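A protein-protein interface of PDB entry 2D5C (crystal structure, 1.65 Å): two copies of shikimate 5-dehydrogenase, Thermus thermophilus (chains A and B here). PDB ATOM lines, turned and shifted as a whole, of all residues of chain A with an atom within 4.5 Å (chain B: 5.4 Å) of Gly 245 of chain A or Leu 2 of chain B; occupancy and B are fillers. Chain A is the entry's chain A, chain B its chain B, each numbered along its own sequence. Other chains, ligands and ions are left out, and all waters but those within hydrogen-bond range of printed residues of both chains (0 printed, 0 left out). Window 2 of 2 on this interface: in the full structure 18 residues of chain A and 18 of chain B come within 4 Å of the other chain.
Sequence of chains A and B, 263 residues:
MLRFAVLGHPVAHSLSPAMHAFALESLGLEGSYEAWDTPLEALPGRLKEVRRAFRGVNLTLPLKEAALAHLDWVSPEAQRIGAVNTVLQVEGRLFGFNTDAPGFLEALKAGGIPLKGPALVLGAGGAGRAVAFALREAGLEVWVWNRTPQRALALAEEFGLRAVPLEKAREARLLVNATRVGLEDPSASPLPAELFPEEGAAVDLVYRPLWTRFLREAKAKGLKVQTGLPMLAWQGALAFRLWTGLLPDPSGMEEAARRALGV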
ATOM      1  N   PHE A 240      31.848  28.140 -20.017  1.00  0.00           N
ATOM      2  CA  PHE A 240      30.855  29.210 -20.016  1.00  0.00           C
ATOM      3  C   PHE A 240      29.448  28.645 -20.236  1.00  0.00           C
ATOM      4  O   PHE A 240      28.480  29.111 -19.624  1.00  0.00           O
ATOM      5  CB  PHE A 240      31.179  30.242 -21.103  1.00  0.00           C
ATOM      6  CG  PHE A 240      30.487  31.557 -20.901  1.00  0.00           C
ATOM      7  CD1 PHE A 240      31.145  32.614 -20.284  1.00  0.00           C
ATOM      8  CD2 PHE A 240      29.162  31.720 -21.303  1.00  0.00           C
ATOM      9  CE1 PHE A 240      30.489  33.837 -20.066  1.00  0.00           C
ATOM     10  CE2 PHE A 240      28.499  32.922 -21.093  1.00  0.00           C
ATOM     11  CZ  PHE A 240      29.161  33.985 -20.474  1.00  0.00           C
ATOM     12  N   ARG A 241      29.327  27.650 -21.113  1.00  0.00           N
ATOM     13  CA  ARG A 241      28.032  27.047 -21.359  1.00  0.00           C
ATOM     14  C   ARG A 241      27.598  26.290 -20.111  1.00  0.00           C
ATOM     15  O   ARG A 241      26.420  26.279 -19.782  1.00  0.00           O
ATOM     16  CB  ARG A 241      28.067  26.104 -22.570  1.00  0.00           C
ATOM     17  CG  ARG A 241      26.692  25.569 -22.945  1.00  0.00           C
ATOM     18  CD  ARG A 241      26.757  24.694 -24.178  1.00  0.00           C
ATOM     19  NE  ARG A 241      27.631  23.546 -23.972  1.00  0.00           N
ATOM     20  CZ  ARG A 241      27.991  22.696 -24.930  1.00  0.00           C
ATOM     21  NH1 ARG A 241      27.555  22.862 -26.174  1.00  0.00           N
ATOM     22  NH2 ARG A 241      28.787  21.673 -24.637  1.00  0.00           N
ATOM     23  N   TRP A 243      28.211  27.103 -17.073  1.00  0.00           N
ATOM     24  CA  TRP A 243      27.752  28.120 -16.135  1.00  0.00           C
ATOM     25  C   TRP A 243      26.441  28.815 -16.494  1.00  0.00           C
ATOM     26  O   TRP A 243      25.652  29.126 -15.609  1.00  0.00           O
ATOM     27  CB  TRP A 243      28.809  29.220 -15.967  1.00  0.00           C
ATOM     28  CG  TRP A 243      30.106  28.760 -15.412  1.00  0.00           C
ATOM     29  CD1 TRP A 243      30.309  27.780 -14.471  1.00  0.00           C
ATOM     30  CD2 TRP A 243      31.399  29.277 -15.743  1.00  0.00           C
ATOM     31  NE1 TRP A 243      31.657  27.656 -14.205  1.00  0.00           N
ATOM     32  CE2 TRP A 243      32.346  28.562 -14.972  1.00  0.00           C
ATOM     33  CE3 TRP A 243      31.848  30.280 -16.618  1.00  0.00           C
ATOM     34  CZ2 TRP A 243      33.720  28.815 -15.051  1.00  0.00           C
ATOM     35  CZ3 TRP A 243      33.227  30.534 -16.695  1.00  0.00           C
ATOM     36  CH2 TRP A 243      34.140  29.802 -15.916  1.00  0.00           C
ATOM     37  N   THR A 244      26.205  29.055 -17.782  1.00  0.00           N
ATOM     38  CA  THR A 244      25.017  29.808 -18.204  1.00  0.00           C
ATOM     39  C   THR A 244      24.001  29.129 -19.114  1.00  0.00           C
ATOM     40  O   THR A 244      22.867  29.599 -19.223  1.00  0.00           O
ATOM     41  CB  THR A 244      25.435  31.066 -18.969  1.00  0.00           C
ATOM     42  OG1 THR A 244      26.053  30.668 -20.206  1.00  0.00           O
ATOM     43  CG2 THR A 244      26.425  31.883 -18.167  1.00  0.00           C
ATOM     44  N   GLY A 245      24.417  28.061 -19.790  1.00  0.00           N
ATOM     45  CA  GLY A 245      23.540  27.391 -20.725  1.00  0.00           C
ATOM     46  C   GLY A 245      23.744  27.988 -22.114  1.00  0.00           C
ATOM     47  O   GLY A 245      23.099  27.586 -23.075  1.00  0.00           O
ATOM     48  N   LEU A 246      24.656  28.951 -22.218  1.00  0.00           N
ATOM     49  CA  LEU A 246      24.939  29.610 -23.497  1.00  0.00           C
ATOM     50  C   LEU A 246      26.360  29.317 -23.964  1.00  0.00           C
ATOM     51  O   LEU A 246      27.287  29.341 -23.164  1.00  0.00           O
ATOM     52  CB  LEU A 246      24.763  31.127 -23.356  1.00  0.00           C
ATOM     53  CG  LEU A 246      23.349  31.626 -23.032  1.00  0.00           C
ATOM     54  CD1 LEU A 246      23.384  33.109 -22.721  1.00  0.00           C
ATOM     55  CD2 LEU A 246      22.432  31.337 -24.200  1.00  0.00           C
ATOM     56  N   LEU A 247      26.528  29.051 -25.259  1.00  0.00           N
ATOM     57  CA  LEU A 247      27.858  28.778 -25.801  1.00  0.00           C
ATOM     58  C   LEU A 247      28.436  29.981 -26.559  1.00  0.00           C
ATOM     59  O   LEU A 247      27.950  30.339 -27.630  1.00  0.00           O
ATOM     60  CB  LEU A 247      27.813  27.565 -26.742  1.00  0.00           C
ATOM     61  CG  LEU A 247      29.153  27.055 -27.308  1.00  0.00           C
ATOM     62  CD1 LEU A 247      30.020  26.474 -26.199  1.00  0.00           C
ATOM     63  CD2 LEU A 247      28.881  25.982 -28.353  1.00  0.00           C
ATOM     64  N   MET B   1      19.891  28.385 -28.125  1.00  0.00           N
ATOM     65  CA  MET B   1      18.893  29.058 -27.243  1.00  0.00           C
ATOM     66  C   MET B   1      18.622  28.268 -25.962  1.00  0.00           C
ATOM     67  O   MET B   1      19.007  27.108 -25.838  1.00  0.00           O
ATOM     68  CB  MET B   1      17.576  29.267 -27.995  1.00  0.00           C
ATOM     69  CG  MET B   1      17.666  30.244 -29.156  1.00  0.00           C
ATOM     70  SD  MET B   1      16.055  30.579 -29.901  1.00  0.00           S
ATOM     71  CE  MET B   1      16.080  29.426 -31.272  1.00  0.00           C
ATOM     72  N   LEU B   2      17.955  28.917 -25.013  1.00  0.00           N
ATOM     73  CA  LEU B   2      17.625  28.303 -23.735  1.00  0.00           C
ATOM     74  C   LEU B   2      16.270  27.614 -23.796  1.00  0.00           C
ATOM     75  O   LEU B   2      15.264  28.234 -24.137  1.00  0.00           O
ATOM     76  CB  LEU B   2      17.608  29.374 -22.646  1.00  0.00           C
ATOM     77  CG  LEU B   2      18.968  30.015 -22.369  1.00  0.00           C
ATOM     78  CD1 LEU B   2      18.787  31.332 -21.634  1.00  0.00           C
ATOM     79  CD2 LEU B   2      19.826  29.038 -21.567  1.00  0.00           C
ATOM     80  N   ARG B   3      16.246  26.331 -23.459  1.00  0.00           N
ATOM     81  CA  ARG B   3      15.005  25.563 -23.471  1.00  0.00           C
ATOM     82  C   ARG B   3      14.621  25.105 -22.067  1.00  0.00           C
ATOM     83  O   ARG B   3      15.351  24.337 -21.429  1.00  0.00           O
ATOM     84  CB  ARG B   3      15.137  24.340 -24.386  1.00  0.00           C
ATOM     85  CG  ARG B   3      15.478  24.671 -25.836  1.00  0.00           C
ATOM     86  CD  ARG B   3      14.443  25.604 -26.446  1.00  0.00           C
ATOM     87  NE  ARG B   3      14.829  26.068 -27.774  1.00  0.00           N
ATOM     88  CZ  ARG B   3      14.155  26.979 -28.470  1.00  0.00           C
ATOM     89  NH1 ARG B   3      13.057  27.524 -27.961  1.00  0.00           N
ATOM     90  NH2 ARG B   3      14.579  27.345 -29.674  1.00  0.00           N
ATOM     91  N   PHE B   4      13.473  25.585 -21.603  1.00  0.00           N
ATOM     92  CA  PHE B   4      12.950  25.243 -20.285  1.00  0.00           C
ATOM     93  C   PHE B   4      11.513  24.740 -20.412  1.00  0.00           C
ATOM     94  O   PHE B   4      10.874  24.883 -21.460  1.00  0.00           O
ATOM     95  CB  PHE B   4      12.934  26.470 -19.370  1.00  0.00           C
ATOM     96  CG  PHE B   4      14.260  27.170 -19.247  1.00  0.00           C
ATOM     97  CD1 PHE B   4      14.420  28.463 -19.733  1.00  0.00           C
ATOM     98  CD2 PHE B   4      15.335  26.562 -18.603  1.00  0.00           C
ATOM     99  CE1 PHE B   4      15.621  29.145 -19.578  1.00  0.00           C
ATOM    100  CE2 PHE B   4      16.550  27.243 -18.441  1.00  0.00           C
ATOM    101  CZ  PHE B   4      16.691  28.535 -18.930  1.00  0.00           C
ATOM    102  N   LEU B  24      12.855  35.719 -19.733  1.00  0.00           N
ATOM    103  CA  LEU B  24      13.740  35.670 -20.892  1.00  0.00           C
ATOM    104  C   LEU B  24      13.823  37.016 -21.591  1.00  0.00           C
ATOM    105  O   LEU B  24      14.912  37.534 -21.842  1.00  0.00           O
ATOM    106  CB  LEU B  24      13.254  34.617 -21.887  1.00  0.00           C
ATOM    107  CG  LEU B  24      13.392  33.164 -21.436  1.00  0.00           C
ATOM    108  CD1 LEU B  24      12.465  32.282 -22.258  1.00  0.00           C
ATOM    109  CD2 LEU B  24      14.841  32.714 -21.568  1.00  0.00           C
ATOM    110  N   LEU B  29      17.407  37.472 -23.238  1.00  0.00           N
ATOM    111  CA  LEU B  29      17.863  36.124 -23.566  1.00  0.00           C
ATOM    112  C   LEU B  29      16.935  35.469 -24.580  1.00  0.00           C
ATOM    113  O   LEU B  29      15.748  35.769 -24.627  1.00  0.00           O
ATOM    114  CB  LEU B  29      17.903  35.267 -22.297  1.00  0.00           C
ATOM    115  CG  LEU B  29      18.892  35.708 -21.213  1.00  0.00           C
ATOM    116  CD1 LEU B  29      18.559  35.026 -19.891  1.00  0.00           C
ATOM    117  CD2 LEU B  29      20.303  35.373 -21.656  1.00  0.00           C
ATOM    118  N   GLU B  30      17.484  34.575 -25.393  1.00  0.00           N
ATOM    119  CA  GLU B  30      16.687  33.870 -26.387  1.00  0.00           C
ATOM    120  C   GLU B  30      16.396  32.472 -25.864  1.00  0.00           C
ATOM    121  O   GLU B  30      17.301  31.763 -25.430  1.00  0.00           O
ATOM    122  CB  GLU B  30      17.441  33.760 -27.709  1.00  0.00           C
ATOM    123  CG  GLU B  30      17.859  35.088 -28.303  1.00  0.00           C
ATOM    124  CD  GLU B  30      18.482  34.923 -29.675  1.00  0.00           C
ATOM    125  OE1 GLU B  30      19.446  34.133 -29.799  1.00  0.00           O
ATOM    126  OE2 GLU B  30      18.006  35.580 -30.626  1.00  0.00           O
ATOM    127  N   GLY B  31      15.133  32.079 -25.902  1.00  0.00           N
ATOM    128  CA  GLY B  31      14.780  30.761 -25.425  1.00  0.00           C
ATOM    129  C   GLY B  31      13.286  30.613 -25.283  1.00  0.00           C
ATOM    130  O   GLY B  31      12.524  31.500 -25.674  1.00  0.00           O
ATOM    131  N   SER B  32      12.866  29.493 -24.713  1.00  0.00           N
ATOM    132  CA  SER B  32      11.454  29.226 -24.524  1.00  0.00           C
ATOM    133  C   SER B  32      11.220  28.464 -23.233  1.00  0.00           C
ATOM    134  O   SER B  32      12.109  27.771 -22.733  1.00  0.00           O
ATOM    135  CB  SER B  32      10.916  28.395 -25.689  1.00  0.00           C
ATOM    136  OG  SER B  32      11.513  27.110 -25.703  1.00  0.00           O
ATOM    137  N   ARG B  55      17.771  22.849 -20.663  1.00  0.00           N
ATOM    138  CA  ARG B  55      18.726  23.376 -19.695  1.00  0.00           C
ATOM    139  C   ARG B  55      18.178  23.156 -18.290  1.00  0.00           C
ATOM    140  O   ARG B  55      18.924  22.916 -17.330  1.00  0.00           O
ATOM    141  CB  ARG B  55      18.946  24.869 -19.941  1.00  0.00           C
ATOM    142  CG  ARG B  55      19.764  25.566 -18.859  1.00  0.00           C
ATOM    143  CD  ARG B  55      21.183  25.033 -18.727  1.00  0.00           C
ATOM    144  NE  ARG B  55      21.939  25.853 -17.779  1.00  0.00           N
ATOM    145  CZ  ARG B  55      23.240  25.735 -17.536  1.00  0.00           C
ATOM    146  NH1 ARG B  55      23.957  24.810 -18.167  1.00  0.00           N
ATOM    147  NH2 ARG B  55      23.828  26.565 -16.674  1.00  0.00           N
ATOM    148  N   PHE B 240      15.183  30.218 -12.265  1.00  0.00           N
ATOM    149  CA  PHE B 240      15.832  30.804 -13.437  1.00  0.00           C
ATOM    150  C   PHE B 240      17.302  31.112 -13.141  1.00  0.00           C
ATOM    151  O   PHE B 240      18.185  30.883 -13.984  1.00  0.00           O
ATOM    152  CB  PHE B 240      15.103  32.091 -13.858  1.00  0.00           C
ATOM    153  CG  PHE B 240      15.342  32.470 -15.290  1.00  0.00           C
ATOM    154  CD1 PHE B 240      14.453  32.069 -16.286  1.00  0.00           C
ATOM    155  CD2 PHE B 240      16.488  33.164 -15.653  1.00  0.00           C
ATOM    156  CE1 PHE B 240      14.710  32.352 -17.624  1.00  0.00           C
ATOM    157  CE2 PHE B 240      16.753  33.450 -16.988  1.00  0.00           C
ATOM    158  CZ  PHE B 240      15.862  33.043 -17.975  1.00  0.00           C
ATOM    159  N   TRP B 243      19.345  28.088 -13.091  1.00  0.00           N
ATOM    160  CA  TRP B 243      19.634  27.644 -14.449  1.00  0.00           C
ATOM    161  C   TRP B 243      20.640  28.468 -15.234  1.00  0.00           C
ATOM    162  O   TRP B 243      21.440  27.910 -15.980  1.00  0.00           O
ATOM    163  CB  TRP B 243      18.354  27.581 -15.294  1.00  0.00           C
ATOM    164  CG  TRP B 243      17.307  26.633 -14.803  1.00  0.00           C
ATOM    165  CD1 TRP B 243      17.502  25.415 -14.234  1.00  0.00           C
ATOM    166  CD2 TRP B 243      15.889  26.830 -14.859  1.00  0.00           C
ATOM    167  NE1 TRP B 243      16.293  24.834 -13.924  1.00  0.00           N
ATOM    168  CE2 TRP B 243      15.286  25.685 -14.297  1.00  0.00           C
ATOM    169  CE3 TRP B 243      15.071  27.866 -15.332  1.00  0.00           C
ATOM    170  CZ2 TRP B 243      13.901  25.546 -14.185  1.00  0.00           C
ATOM    171  CZ3 TRP B 243      13.690  27.728 -15.225  1.00  0.00           C
ATOM    172  CH2 TRP B 243      13.117  26.571 -14.652  1.00  0.00           C
ATOM    173  N   THR B 244      20.610  29.786 -15.058  1.00  0.00           N
ATOM    174  CA  THR B 244      21.444  30.676 -15.851  1.00  0.00           C
ATOM    175  C   THR B 244      22.436  31.578 -15.143  1.00  0.00           C
ATOM    176  O   THR B 244      23.375  32.069 -15.766  1.00  0.00           O
ATOM    177  CB  THR B 244      20.544  31.611 -16.678  1.00  0.00           C
ATOM    178  OG1 THR B 244      19.876  32.523 -15.786  1.00  0.00           O
ATOM    179  CG2 THR B 244      19.498  30.801 -17.460  1.00  0.00           C
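The backbone carbonyl oxygen (O) of Trp 243 of chain A sits at hydrogen-bond distance from the guanidinium group (NH2) of Arg 55 of chain B (3.3 Å).
The backbone carbonyl oxygen of Arg 241 of chain A is in hydrogen-bond range of the guanidinium group of Arg 55 of chain B.
N of Ser 32 of chain B lies within hydrogen-bond range of O of Leu 2 of chain B, 2.8 Å away.
O of Arg 3 of chain B sits at hydrogen-bond distance from N of Arg 55 of chain B (2.9 Å).
The side-chain hydroxyl of Thr 244 of chain A lies within hydrogen-bond range of the backbone NH of Leu 246 of chain A (3.0 Å).
The backbone carbonyl oxygen of Phe 240 of chain A sits at hydrogen-bond distance from the side-chain hydroxyl of Thr 244 of chain A (2.9 Å).
The backbone NH (N) of Arg 241 of chain A lies close to the backbone carbonyl oxygen (O) of Leu 246 of chain A.
The backbone carbonyl oxygen (O) of Leu 24 of chain B lies within hydrogen-bond range of the backbone NH (N) of Leu 29 of chain B (2.9 Å).
Among the printed residues, merely in contact across the chains: Gly 245 of chain A with Arg 55 of chain B (3.4 Å), Thr 244 of chain A with Arg 55 of chain B (3.5 Å), Thr 244 of chain A with Thr 244 of chain B (3.7 Å), Trp 243 of chain A with Thr 244 of chain B (3.7 Å), Thr 244 of chain A with Leu 2 of chain B (3.9 Å), Gly 245 of chain A with Leu 2 of chain B (3.9 Å), Thr 244 of chain A with Trp 243 of chain B (3.9 Å) and Leu 246 of chain A with Leu 29 of chain B (3.97 Å).
Gly 245 of chain A touches just these residues of chain B: Leu 2 (3.9 Å) and Arg 55 (3.4 Å).
Of the printed residues of chain A, Leu 2 of chain B touches Thr 244 (3.9 Å) and Gly 245 (3.9 Å).
Of the printed residues of chain A, Arg 55 of chain B touches Arg 241 (3.3 Å), Trp 243 (3.3 Å), Thr 244 (3.5 Å) and Gly 245 (3.4 Å).
Of the printed residues of chain B, Thr 244 of chain A touches Leu 2, Arg 55, Trp 243 and Thr 244.
Printed residues of chain B within 4 Å of Arg 241 of chain A: Arg 55.
Phe 240 of chain A touches none of the printed residues of chain B.
Leu 24 of chain B touches none of the printed residues of chain A.
The nearest residue of chain A that does not touch Leu 2 of chain B is Leu 246 of chain A (4.1 Å).
The nearest printed residue of chain A that does not touch Arg 55 of chain B is Leu 246 of chain A (5.8 Å).
Of the 13 printed residues of chain B, 5 touch a printed residue of chain A.
Hydrophobic or aromatic side chains of chain A that line the printed part of chain B: Leu 246.
Trp 243 of chain A touches Thr 244 of chain B, and with the chains exchanged Thr 244 of chain A touches Trp 243 of chain B.
Thr 244 of chain A touches its own counterpart, Thr 244 of chain B.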
